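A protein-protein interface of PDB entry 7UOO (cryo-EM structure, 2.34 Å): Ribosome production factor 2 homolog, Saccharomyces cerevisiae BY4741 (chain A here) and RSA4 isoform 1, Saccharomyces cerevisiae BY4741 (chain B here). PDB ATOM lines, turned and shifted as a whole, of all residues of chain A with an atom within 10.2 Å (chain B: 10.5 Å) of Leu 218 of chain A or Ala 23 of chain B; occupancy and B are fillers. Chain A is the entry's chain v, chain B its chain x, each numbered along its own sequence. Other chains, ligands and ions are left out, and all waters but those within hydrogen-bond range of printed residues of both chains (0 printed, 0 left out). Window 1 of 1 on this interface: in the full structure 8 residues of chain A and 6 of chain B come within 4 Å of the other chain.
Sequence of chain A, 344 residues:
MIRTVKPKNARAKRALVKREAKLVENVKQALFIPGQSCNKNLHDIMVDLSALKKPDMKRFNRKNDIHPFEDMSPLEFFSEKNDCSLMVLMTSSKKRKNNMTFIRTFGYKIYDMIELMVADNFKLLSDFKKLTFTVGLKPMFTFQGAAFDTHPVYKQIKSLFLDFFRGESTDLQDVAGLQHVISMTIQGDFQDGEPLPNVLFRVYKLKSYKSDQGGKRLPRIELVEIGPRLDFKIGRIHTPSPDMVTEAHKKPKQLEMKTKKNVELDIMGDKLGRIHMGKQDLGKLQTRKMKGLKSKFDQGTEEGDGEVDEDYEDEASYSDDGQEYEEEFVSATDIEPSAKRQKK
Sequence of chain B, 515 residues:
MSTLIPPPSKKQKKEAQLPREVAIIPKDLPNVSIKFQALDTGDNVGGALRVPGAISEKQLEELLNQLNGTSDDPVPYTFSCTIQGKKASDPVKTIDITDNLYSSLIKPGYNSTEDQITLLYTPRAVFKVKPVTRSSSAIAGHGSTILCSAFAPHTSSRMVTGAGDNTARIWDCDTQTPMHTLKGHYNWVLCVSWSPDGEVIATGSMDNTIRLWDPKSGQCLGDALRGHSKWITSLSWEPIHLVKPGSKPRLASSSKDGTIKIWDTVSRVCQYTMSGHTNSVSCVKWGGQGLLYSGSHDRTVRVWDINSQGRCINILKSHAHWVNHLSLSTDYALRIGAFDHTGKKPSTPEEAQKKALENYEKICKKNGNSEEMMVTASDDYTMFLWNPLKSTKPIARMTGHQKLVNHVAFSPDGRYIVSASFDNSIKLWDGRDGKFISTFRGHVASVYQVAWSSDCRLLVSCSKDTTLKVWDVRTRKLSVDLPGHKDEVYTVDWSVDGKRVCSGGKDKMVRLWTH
Hydrophobic or aromatic side chains of chain A within 4 Å of the printed part of chain B: Leu 218. Hydrophobic or aromatic side chains of chain B within 4 Å of the printed part of chain A: Val 22 and Ile 25. Among the printed residues, 6 pairs touch across the chains.
The side-chain hydroxyl (OG) of Ser 211 of chain A lies within hydrogen-bond range of the backbone carbonyl oxygen (O) of Leu 218 of chain A, at 3.0 Å.
Ile 25 of chain B touches Gln 213 of chain A. Gly 215 of chain A touches Ile 25 of chain B (N to CD1, 3.9 Å). Asp 99 of chain B touches Lys 216 of chain A (OD1 to CD, 3.3 Å). Arg 217 of chain A touches Asp 99 of chain B. CD1 of Leu 218 of chain A touches CG1 of Val 22 of chain B, at 3.7 Å. Ala 23 of chain B touches Leu 218 of chain A (O to CD1, 3.8 Å).
Of the printed residues of chain B, Gln 213 of chain A touches Ile 25 (3.9 Å). No residue of chain B comes within 4 Å of Gly 214 of chain A. Of chain B, only Ile 25 (3.9 Å) comes within 4 Å of Gly 215 of chain A. Of the printed residues of chain B, Lys 216 of chain A touches Asp 99. Of the printed residues of chain B, Arg 217 of chain A touches Asp 99 (3.9 Å). Of the printed residues of chain B, Leu 218 of chain A touches Val 22 and Ala 23. Arg 220 of chain A touches none of the printed residues of chain B. Val 22 of chain B touches just one residue of chain A: Leu 218 (3.7 Å). Printed residues of chain A within 4 Å of Ala 23 of chain B: Leu 218 (3.8 Å). No residue of chain A comes within 4 Å of Ile 24 of chain B. Of the printed residues of chain A, Ile 25 of chain B touches Gln 213 (3.9 Å) and Gly 215 (3.9 Å). Of the printed residues of chain A, Asp 99 of chain B touches Lys 216 (3.3 Å) and Arg 217 (3.9 Å). Tyr 102 of chain B touches none of the printed residues of chain A. The nearest residue of chain B that does not touch Leu 218 of chain A is Ile 24 of chain B (4.1 Å).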
ATOM      1  N   VAL A 175      -9.305  24.175  24.263  1.00  0.00           N
ATOM      2  CA  VAL A 175      -9.327  23.162  25.308  1.00  0.00           C
ATOM      3  C   VAL A 175      -7.924  22.863  25.824  1.00  0.00           C
ATOM      4  O   VAL A 175      -7.771  22.342  26.935  1.00  0.00           O
ATOM      5  CB  VAL A 175     -10.025  21.897  24.776  1.00  0.00           C
ATOM      6  CG1 VAL A 175     -10.458  20.998  25.914  1.00  0.00           C
ATOM      7  CG2 VAL A 175     -11.225  22.284  23.933  1.00  0.00           C
ATOM      8  N   LYS A 207      -5.305  16.839  35.426  1.00  0.00           N
ATOM      9  CA  LYS A 207      -4.790  15.703  34.674  1.00  0.00           C
ATOM     10  C   LYS A 207      -5.980  14.890  34.192  1.00  0.00           C
ATOM     11  O   LYS A 207      -6.770  14.405  35.008  1.00  0.00           O
ATOM     12  CB  LYS A 207      -3.853  14.842  35.525  1.00  0.00           C
ATOM     13  CG  LYS A 207      -2.457  15.412  35.687  1.00  0.00           C
ATOM     14  CD  LYS A 207      -1.607  14.545  36.602  1.00  0.00           C
ATOM     15  CE  LYS A 207      -0.167  15.030  36.637  1.00  0.00           C
ATOM     16  NZ  LYS A 207      -0.070  16.476  36.975  1.00  0.00           N
ATOM     17  N   SER A 208      -6.116  14.751  32.880  1.00  0.00           N
ATOM     18  CA  SER A 208      -7.234  14.030  32.289  1.00  0.00           C
ATOM     19  C   SER A 208      -6.822  12.603  31.961  1.00  0.00           C
ATOM     20  O   SER A 208      -5.696  12.352  31.523  1.00  0.00           O
ATOM     21  CB  SER A 208      -7.739  14.739  31.031  1.00  0.00           C
ATOM     22  OG  SER A 208      -6.675  15.033  30.144  1.00  0.00           O
ATOM     23  N   TYR A 209      -7.741  11.669  32.186  1.00  0.00           N
ATOM     24  CA  TYR A 209      -7.511  10.257  31.937  1.00  0.00           C
ATOM     25  C   TYR A 209      -8.719   9.673  31.222  1.00  0.00           C
ATOM     26  O   TYR A 209      -9.825  10.217  31.287  1.00  0.00           O
ATOM     27  CB  TYR A 209      -7.252   9.484  33.239  1.00  0.00           C
ATOM     28  CG  TYR A 209      -6.145  10.055  34.097  1.00  0.00           C
ATOM     29  CD1 TYR A 209      -6.411  11.032  35.048  1.00  0.00           C
ATOM     30  CD2 TYR A 209      -4.836   9.613  33.963  1.00  0.00           C
ATOM     31  CE1 TYR A 209      -5.403  11.556  35.835  1.00  0.00           C
ATOM     32  CE2 TYR A 209      -3.823  10.128  34.748  1.00  0.00           C
ATOM     33  CZ  TYR A 209      -4.112  11.100  35.681  1.00  0.00           C
ATOM     34  OH  TYR A 209      -3.108  11.618  36.464  1.00  0.00           O
ATOM     35  N   LYS A 210      -8.495   8.563  30.523  1.00  0.00           N
ATOM     36  CA  LYS A 210      -9.592   7.853  29.884  1.00  0.00           C
ATOM     37  C   LYS A 210     -10.537   7.299  30.942  1.00  0.00           C
ATOM     38  O   LYS A 210     -10.104   6.814  31.991  1.00  0.00           O
ATOM     39  CB  LYS A 210      -9.059   6.724  29.004  1.00  0.00           C
ATOM     40  CG  LYS A 210     -10.067   6.206  27.993  1.00  0.00           C
ATOM     41  CD  LYS A 210     -10.178   7.142  26.800  1.00  0.00           C
ATOM     42  CE  LYS A 210     -11.468   6.912  26.032  1.00  0.00           C
ATOM     43  NZ  LYS A 210     -11.716   5.470  25.766  1.00  0.00           N
ATOM     44  N   SER A 211     -11.837   7.373  30.665  1.00  0.00           N
ATOM     45  CA  SER A 211     -12.851   7.081  31.669  1.00  0.00           C
ATOM     46  C   SER A 211     -13.466   5.696  31.545  1.00  0.00           C
ATOM     47  O   SER A 211     -13.856   5.120  32.567  1.00  0.00           O
ATOM     48  CB  SER A 211     -13.969   8.126  31.607  1.00  0.00           C
ATOM     49  OG  SER A 211     -14.549   8.178  30.317  1.00  0.00           O
ATOM     50  N   ASP A 212     -13.603   5.170  30.326  1.00  0.00           N
ATOM     51  CA  ASP A 212     -14.195   3.872  29.996  1.00  0.00           C
ATOM     52  C   ASP A 212     -15.687   3.806  30.319  1.00  0.00           C
ATOM     53  O   ASP A 212     -16.317   2.772  30.070  1.00  0.00           O
ATOM     54  CB  ASP A 212     -13.474   2.700  30.684  1.00  0.00           C
ATOM     55  CG  ASP A 212     -13.617   1.395  29.924  1.00  0.00           C
ATOM     56  OD1 ASP A 212     -14.156   1.415  28.799  1.00  0.00           O
ATOM     57  OD2 ASP A 212     -13.190   0.348  30.455  1.00  0.00           O
ATOM     58  N   GLN A 213     -16.277   4.873  30.856  1.00  0.00           N
ATOM     59  CA  GLN A 213     -17.708   4.936  31.106  1.00  0.00           C
ATOM     60  C   GLN A 213     -18.347   6.219  30.600  1.00  0.00           C
ATOM     61  O   GLN A 213     -19.577   6.332  30.648  1.00  0.00           O
ATOM     62  CB  GLN A 213     -18.006   4.789  32.607  1.00  0.00           C
ATOM     63  CG  GLN A 213     -17.744   3.396  33.160  1.00  0.00           C
ATOM     64  CD  GLN A 213     -18.182   3.246  34.606  1.00  0.00           C
ATOM     65  OE1 GLN A 213     -18.518   4.226  35.271  1.00  0.00           O
ATOM     66  NE2 GLN A 213     -18.185   2.012  35.097  1.00  0.00           N
ATOM     67  N   GLY A 214     -17.562   7.186  30.135  1.00  0.00           N
ATOM     68  CA  GLY A 214     -18.098   8.386  29.529  1.00  0.00           C
ATOM     69  C   GLY A 214     -17.752   8.474  28.058  1.00  0.00           C
ATOM     70  O   GLY A 214     -17.786   9.557  27.466  1.00  0.00           O
ATOM     71  N   GLY A 215     -17.414   7.333  27.458  1.00  0.00           N
ATOM     72  CA  GLY A 215     -17.021   7.319  26.065  1.00  0.00           C
ATOM     73  C   GLY A 215     -15.658   7.957  25.858  1.00  0.00           C
ATOM     74  O   GLY A 215     -14.798   7.966  26.741  1.00  0.00           O
ATOM     75  N   LYS A 216     -15.460   8.495  24.658  1.00  0.00           N
ATOM     76  CA  LYS A 216     -14.235   9.201  24.311  1.00  0.00           C
ATOM     77  C   LYS A 216     -14.404  10.712  24.356  1.00  0.00           C
ATOM     78  O   LYS A 216     -13.536  11.438  23.864  1.00  0.00           O
ATOM     79  CB  LYS A 216     -13.748   8.763  22.929  1.00  0.00           C
ATOM     80  CG  LYS A 216     -14.743   9.014  21.808  1.00  0.00           C
ATOM     81  CD  LYS A 216     -14.338   8.279  20.537  1.00  0.00           C
ATOM     82  CE  LYS A 216     -12.967   8.720  20.044  1.00  0.00           C
ATOM     83  NZ  LYS A 216     -12.950  10.152  19.643  1.00  0.00           N
ATOM     84  N   ARG A 217     -15.501  11.201  24.933  1.00  0.00           N
ATOM     85  CA  ARG A 217     -15.783  12.628  24.988  1.00  0.00           C
ATOM     86  C   ARG A 217     -15.618  13.236  26.372  1.00  0.00           C
ATOM     87  O   ARG A 217     -15.289  14.420  26.470  1.00  0.00           O
ATOM     88  CB  ARG A 217     -17.211  12.907  24.500  1.00  0.00           C
ATOM     89  CG  ARG A 217     -17.609  12.139  23.250  1.00  0.00           C
ATOM     90  CD  ARG A 217     -16.714  12.469  22.065  1.00  0.00           C
ATOM     91  NE  ARG A 217     -16.702  13.895  21.761  1.00  0.00           N
ATOM     92  CZ  ARG A 217     -17.642  14.521  21.068  1.00  0.00           C
ATOM     93  NH1 ARG A 217     -18.703  13.880  20.605  1.00  0.00           N
ATOM     94  NH2 ARG A 217     -17.517  15.825  20.835  1.00  0.00           N
ATOM     95  N   LEU A 218     -15.830  12.463  27.439  1.00  0.00           N
ATOM     96  CA  LEU A 218     -15.812  12.970  28.811  1.00  0.00           C
ATOM     97  C   LEU A 218     -14.718  12.260  29.599  1.00  0.00           C
ATOM     98  O   LEU A 218     -14.954  11.187  30.176  1.00  0.00           O
ATOM     99  CB  LEU A 218     -17.170  12.780  29.480  1.00  0.00           C
ATOM    100  CG  LEU A 218     -18.377  13.349  28.737  1.00  0.00           C
ATOM    101  CD1 LEU A 218     -19.650  13.038  29.498  1.00  0.00           C
ATOM    102  CD2 LEU A 218     -18.223  14.847  28.528  1.00  0.00           C
ATOM    103  N   PRO A 219     -13.517  12.821  29.657  1.00  0.00           N
ATOM    104  CA  PRO A 219     -12.430  12.176  30.396  1.00  0.00           C
ATOM    105  C   PRO A 219     -12.587  12.331  31.902  1.00  0.00           C
ATOM    106  O   PRO A 219     -13.255  13.236  32.403  1.00  0.00           O
ATOM    107  CB  PRO A 219     -11.186  12.919  29.899  1.00  0.00           C
ATOM    108  CG  PRO A 219     -11.694  14.276  29.577  1.00  0.00           C
ATOM    109  CD  PRO A 219     -13.088  14.089  29.042  1.00  0.00           C
ATOM    110  N   ARG A 220     -11.950  11.411  32.622  1.00  0.00           N
ATOM    111  CA  ARG A 220     -11.866  11.497  34.073  1.00  0.00           C
ATOM    112  C   ARG A 220     -10.831  12.543  34.462  1.00  0.00           C
ATOM    113  O   ARG A 220      -9.721  12.565  33.920  1.00  0.00           O
ATOM    114  CB  ARG A 220     -11.502  10.138  34.666  1.00  0.00           C
ATOM    115  CG  ARG A 220     -11.206  10.155  36.157  1.00  0.00           C
ATOM    116  CD  ARG A 220     -12.467  10.324  36.990  1.00  0.00           C
ATOM    117  NE  ARG A 220     -12.182  10.208  38.415  1.00  0.00           N
ATOM    118  CZ  ARG A 220     -13.105  10.162  39.365  1.00  0.00           C
ATOM    119  NH1 ARG A 220     -14.395  10.212  39.080  1.00  0.00           N
ATOM    120  NH2 ARG A 220     -12.723  10.061  40.634  1.00  0.00           N
ATOM    121  N   ILE A 221     -11.193  13.408  35.402  1.00  0.00           N
ATOM    122  CA  ILE A 221     -10.348  14.517  35.828  1.00  0.00           C
ATOM    123  C   ILE A 221      -9.701  14.160  37.158  1.00  0.00           C
ATOM    124  O   ILE A 221     -10.305  13.473  37.990  1.00  0.00           O
ATOM    125  CB  ILE A 221     -11.170  15.816  35.933  1.00  0.00           C
ATOM    126  CG1 ILE A 221     -11.985  16.030  34.655  1.00  0.00           C
ATOM    127  CG2 ILE A 221     -10.270  17.014  36.175  1.00  0.00           C
ATOM    128  CD1 ILE A 221     -11.141  16.184  33.414  1.00  0.00           C
ATOM    129  N   ARG B  20     -26.490  23.306  30.176  1.00  0.00           N
ATOM    130  CA  ARG B  20     -26.389  22.365  29.072  1.00  0.00           C
ATOM    131  C   ARG B  20     -26.657  20.940  29.541  1.00  0.00           C
ATOM    132  O   ARG B  20     -26.582  20.621  30.731  1.00  0.00           O
ATOM    133  CB  ARG B  20     -25.005  22.444  28.425  1.00  0.00           C
ATOM    134  CG  ARG B  20     -24.670  23.789  27.797  1.00  0.00           C
ATOM    135  CD  ARG B  20     -25.412  23.996  26.486  1.00  0.00           C
ATOM    136  NE  ARG B  20     -25.318  22.826  25.624  1.00  0.00           N
ATOM    137  CZ  ARG B  20     -25.656  22.808  24.342  1.00  0.00           C
ATOM    138  NH1 ARG B  20     -26.084  23.898  23.725  1.00  0.00           N
ATOM    139  NH2 ARG B  20     -25.559  21.670  23.660  1.00  0.00           N
ATOM    140  N   GLU B  21     -26.969  20.077  28.580  1.00  0.00           N
ATOM    141  CA  GLU B  21     -27.184  18.662  28.834  1.00  0.00           C
ATOM    142  C   GLU B  21     -25.906  17.888  28.539  1.00  0.00           C
ATOM    143  O   GLU B  21     -25.177  18.211  27.597  1.00  0.00           O
ATOM    144  CB  GLU B  21     -28.345  18.123  27.993  1.00  0.00           C
ATOM    145  CG  GLU B  21     -28.283  18.477  26.515  1.00  0.00           C
ATOM    146  CD  GLU B  21     -27.483  17.475  25.703  1.00  0.00           C
ATOM    147  OE1 GLU B  21     -27.675  16.257  25.902  1.00  0.00           O
ATOM    148  OE2 GLU B  21     -26.650  17.910  24.879  1.00  0.00           O
ATOM    149  N   VAL B  22     -25.635  16.874  29.353  1.00  0.00           N
ATOM    150  CA  VAL B  22     -24.411  16.089  29.257  1.00  0.00           C
ATOM    151  C   VAL B  22     -24.757  14.744  28.638  1.00  0.00           C
ATOM    152  O   VAL B  22     -25.569  13.988  29.188  1.00  0.00           O
ATOM    153  CB  VAL B  22     -23.746  15.911  30.630  1.00  0.00           C
ATOM    154  CG1 VAL B  22     -22.395  15.242  30.481  1.00  0.00           C
ATOM    155  CG2 VAL B  22     -23.605  17.252  31.325  1.00  0.00           C
ATOM    156  N   ALA B  23     -24.140  14.442  27.496  1.00  0.00           N
ATOM    157  CA  ALA B  23     -24.369  13.172  26.820  1.00  0.00           C
ATOM    158  C   ALA B  23     -23.677  12.044  27.570  1.00  0.00           C
ATOM    159  O   ALA B  23     -22.495  11.769  27.340  1.00  0.00           O
ATOM    160  CB  ALA B  23     -23.879  13.234  25.373  1.00  0.00           C
ATOM    161  N   ILE B  24     -24.404  11.389  28.468  1.00  0.00           N
ATOM    162  CA  ILE B  24     -23.854  10.334  29.307  1.00  0.00           C
ATOM    163  C   ILE B  24     -24.460   9.005  28.878  1.00  0.00           C
ATOM    164  O   ILE B  24     -25.572   8.947  28.339  1.00  0.00           O
ATOM    165  CB  ILE B  24     -24.107  10.619  30.805  1.00  0.00           C
ATOM    166  CG1 ILE B  24     -23.154   9.807  31.681  1.00  0.00           C
ATOM    167  CG2 ILE B  24     -25.556  10.349  31.180  1.00  0.00           C
ATOM    168  CD1 ILE B  24     -21.695  10.129  31.453  1.00  0.00           C
ATOM    169  N   ILE B  25     -23.703   7.934  29.085  1.00  0.00           N
ATOM    170  CA  ILE B  25     -24.138   6.584  28.746  1.00  0.00           C
ATOM    171  C   ILE B  25     -24.966   6.051  29.911  1.00  0.00           C
ATOM    172  O   ILE B  25     -24.448   5.980  31.037  1.00  0.00           O
ATOM    173  CB  ILE B  25     -22.945   5.666  28.461  1.00  0.00           C
ATOM    174  CG1 ILE B  25     -22.063   6.260  27.362  1.00  0.00           C
ATOM    175  CG2 ILE B  25     -23.424   4.276  28.070  1.00  0.00           C
ATOM    176  CD1 ILE B  25     -20.812   5.457  27.085  1.00  0.00           C
ATOM    177  N   PRO B  26     -26.233   5.695  29.700  1.00  0.00           N
ATOM    178  CA  PRO B  26     -27.024   5.110  30.789  1.00  0.00           C
ATOM    179  C   PRO B  26     -26.441   3.784  31.257  1.00  0.00           C
ATOM    180  O   PRO B  26     -25.989   2.964  30.455  1.00  0.00           O
ATOM    181  CB  PRO B  26     -28.411   4.925  30.161  1.00  0.00           C
ATOM    182  CG  PRO B  26     -28.441   5.871  29.007  1.00  0.00           C
ATOM    183  CD  PRO B  26     -27.037   5.914  28.487  1.00  0.00           C
ATOM    184  N   LYS B  27     -26.455   3.582  32.574  1.00  0.00           N
ATOM    185  CA  LYS B  27     -25.980   2.326  33.143  1.00  0.00           C
ATOM    186  C   LYS B  27     -26.997   1.205  32.971  1.00  0.00           C
ATOM    187  O   LYS B  27     -26.616   0.030  32.918  1.00  0.00           O
ATOM    188  CB  LYS B  27     -25.649   2.509  34.622  1.00  0.00           C
ATOM    189  CG  LYS B  27     -24.741   3.689  34.907  1.00  0.00           C
ATOM    190  CD  LYS B  27     -24.551   3.890  36.401  1.00  0.00           C
ATOM    191  CE  LYS B  27     -23.656   5.082  36.687  1.00  0.00           C
ATOM    192  NZ  LYS B  27     -23.437   5.271  38.150  1.00  0.00           N
ATOM    193  N   LEU B  29     -28.669   0.491  30.354  1.00  0.00           N
ATOM    194  CA  LEU B  29     -28.879   0.309  28.927  1.00  0.00           C
ATOM    195  C   LEU B  29     -29.027  -1.173  28.613  1.00  0.00           C
ATOM    196  O   LEU B  29     -28.096  -1.947  28.874  1.00  0.00           O
ATOM    197  CB  LEU B  29     -27.712   0.907  28.152  1.00  0.00           C
ATOM    198  CG  LEU B  29     -28.028   1.612  26.836  1.00  0.00           C
ATOM    199  CD1 LEU B  29     -29.206   2.555  27.006  1.00  0.00           C
ATOM    200  CD2 LEU B  29     -26.803   2.373  26.369  1.00  0.00           C
ATOM    201  N   ASP B  99     -18.853   6.728  17.344  1.00  0.00           N
ATOM    202  CA  ASP B  99     -18.202   6.423  18.611  1.00  0.00           C
ATOM    203  C   ASP B  99     -18.782   5.195  19.291  1.00  0.00           C
ATOM    204  O   ASP B  99     -18.034   4.272  19.636  1.00  0.00           O
ATOM    205  CB  ASP B  99     -18.289   7.635  19.553  1.00  0.00           C
ATOM    206  CG  ASP B  99     -17.568   8.850  19.005  1.00  0.00           C
ATOM    207  OD1 ASP B  99     -16.633   8.673  18.194  1.00  0.00           O
ATOM    208  OD2 ASP B  99     -17.933   9.982  19.382  1.00  0.00           O
ATOM    209  N   ASN B 100     -20.097   5.152  19.498  1.00  0.00           N
ATOM    210  CA  ASN B 100     -20.722   4.012  20.148  1.00  0.00           C
ATOM    211  C   ASN B 100     -22.152   3.871  19.648  1.00  0.00           C
ATOM    212  O   ASN B 100     -22.738   4.809  19.097  1.00  0.00           O
ATOM    213  CB  ASN B 100     -20.690   4.141  21.678  1.00  0.00           C
ATOM    214  CG  ASN B 100     -21.558   5.270  22.187  1.00  0.00           C
ATOM    215  OD1 ASN B 100     -21.162   6.435  22.158  1.00  0.00           O
ATOM    216  ND2 ASN B 100     -22.747   4.931  22.667  1.00  0.00           N
ATOM    217  N   TYR B 102     -25.081   3.470  21.161  1.00  0.00           N
ATOM    218  CA  TYR B 102     -26.135   4.268  21.780  1.00  0.00           C
ATOM    219  C   TYR B 102     -26.147   5.690  21.234  1.00  0.00           C
ATOM    220  O   TYR B 102     -27.208   6.228  20.902  1.00  0.00           O
ATOM    221  CB  TYR B 102     -25.970   4.279  23.299  1.00  0.00           C
ATOM    222  CG  TYR B 102     -26.990   5.145  24.001  1.00  0.00           C
ATOM    223  CD1 TYR B 102     -28.301   4.715  24.156  1.00  0.00           C
ATOM    224  CD2 TYR B 102     -26.646   6.393  24.503  1.00  0.00           C
ATOM    225  CE1 TYR B 102     -29.241   5.502  24.791  1.00  0.00           C
ATOM    226  CE2 TYR B 102     -27.581   7.189  25.143  1.00  0.00           C
ATOM    227  CZ  TYR B 102     -28.876   6.736  25.284  1.00  0.00           C
ATOM    228  OH  TYR B 102     -29.813   7.517  25.916  1.00  0.00           O
ATOM    229  N   SER B 103     -24.973   6.314  21.127  1.00  0.00           N
ATOM    230  CA  SER B 103     -24.906   7.670  20.597  1.00  0.00           C
ATOM    231  C   SER B 103     -25.105   7.709  19.091  1.00  0.00           C
ATOM    232  O   SER B 103     -25.380   8.782  18.542  1.00  0.00           O
ATOM    233  CB  SER B 103     -23.570   8.316  20.961  1.00  0.00           C
ATOM    234  OG  SER B 103     -22.487   7.616  20.375  1.00  0.00           O
ATOM    235  N   SER B 104     -24.974   6.571  18.411  1.00  0.00           N
ATOM    236  CA  SER B 104     -25.151   6.531  16.967  1.00  0.00           C
ATOM    237  C   SER B 104     -26.609   6.325  16.564  1.00  0.00           C
ATOM    238  O   SER B 104     -27.117   7.033  15.691  1.00  0.00           O
ATOM    239  CB  SER B 104     -24.277   5.424  16.369  1.00  0.00           C
ATOM    240  OG  SER B 104     -22.925   5.583  16.758  1.00  0.00           O
ATOM    241  N   LYS B 107     -29.739   7.062  20.611  1.00  0.00           N
ATOM    242  CA  LYS B 107     -29.922   8.466  20.978  1.00  0.00           C
ATOM    243  C   LYS B 107     -30.736   9.260  19.956  1.00  0.00           C
ATOM    244  O   LYS B 107     -31.601  10.044  20.387  1.00  0.00           O
ATOM    245  CB  LYS B 107     -28.560   9.124  21.243  1.00  0.00           C
ATOM    246  CG  LYS B 107     -28.640  10.610  21.558  1.00  0.00           C
ATOM    247  CD  LYS B 107     -27.261  11.231  21.674  1.00  0.00           C
ATOM    248  CE  LYS B 107     -27.343  12.747  21.758  1.00  0.00           C
ATOM    249  NZ  LYS B 107     -25.994  13.378  21.733  1.00  0.00           N
ATOM    250  N   PRO B 108     -30.530   9.138  18.635  1.00  0.00           N
ATOM    251  CA  PRO B 108     -31.500   9.745  17.708  1.00  0.00           C
ATOM    252  C   PRO B 108     -32.907   9.190  17.852  1.00  0.00           C
ATOM    253  O   PRO B 108     -33.877   9.906  17.570  1.00  0.00           O
ATOM    254  CB  PRO B 108     -30.909   9.430  16.327  1.00  0.00           C
ATOM    255  CG  PRO B 108     -29.458   9.323  16.569  1.00  0.00           C
ATOM    256  CD  PRO B 108     -29.335   8.662  17.908  1.00  0.00           C
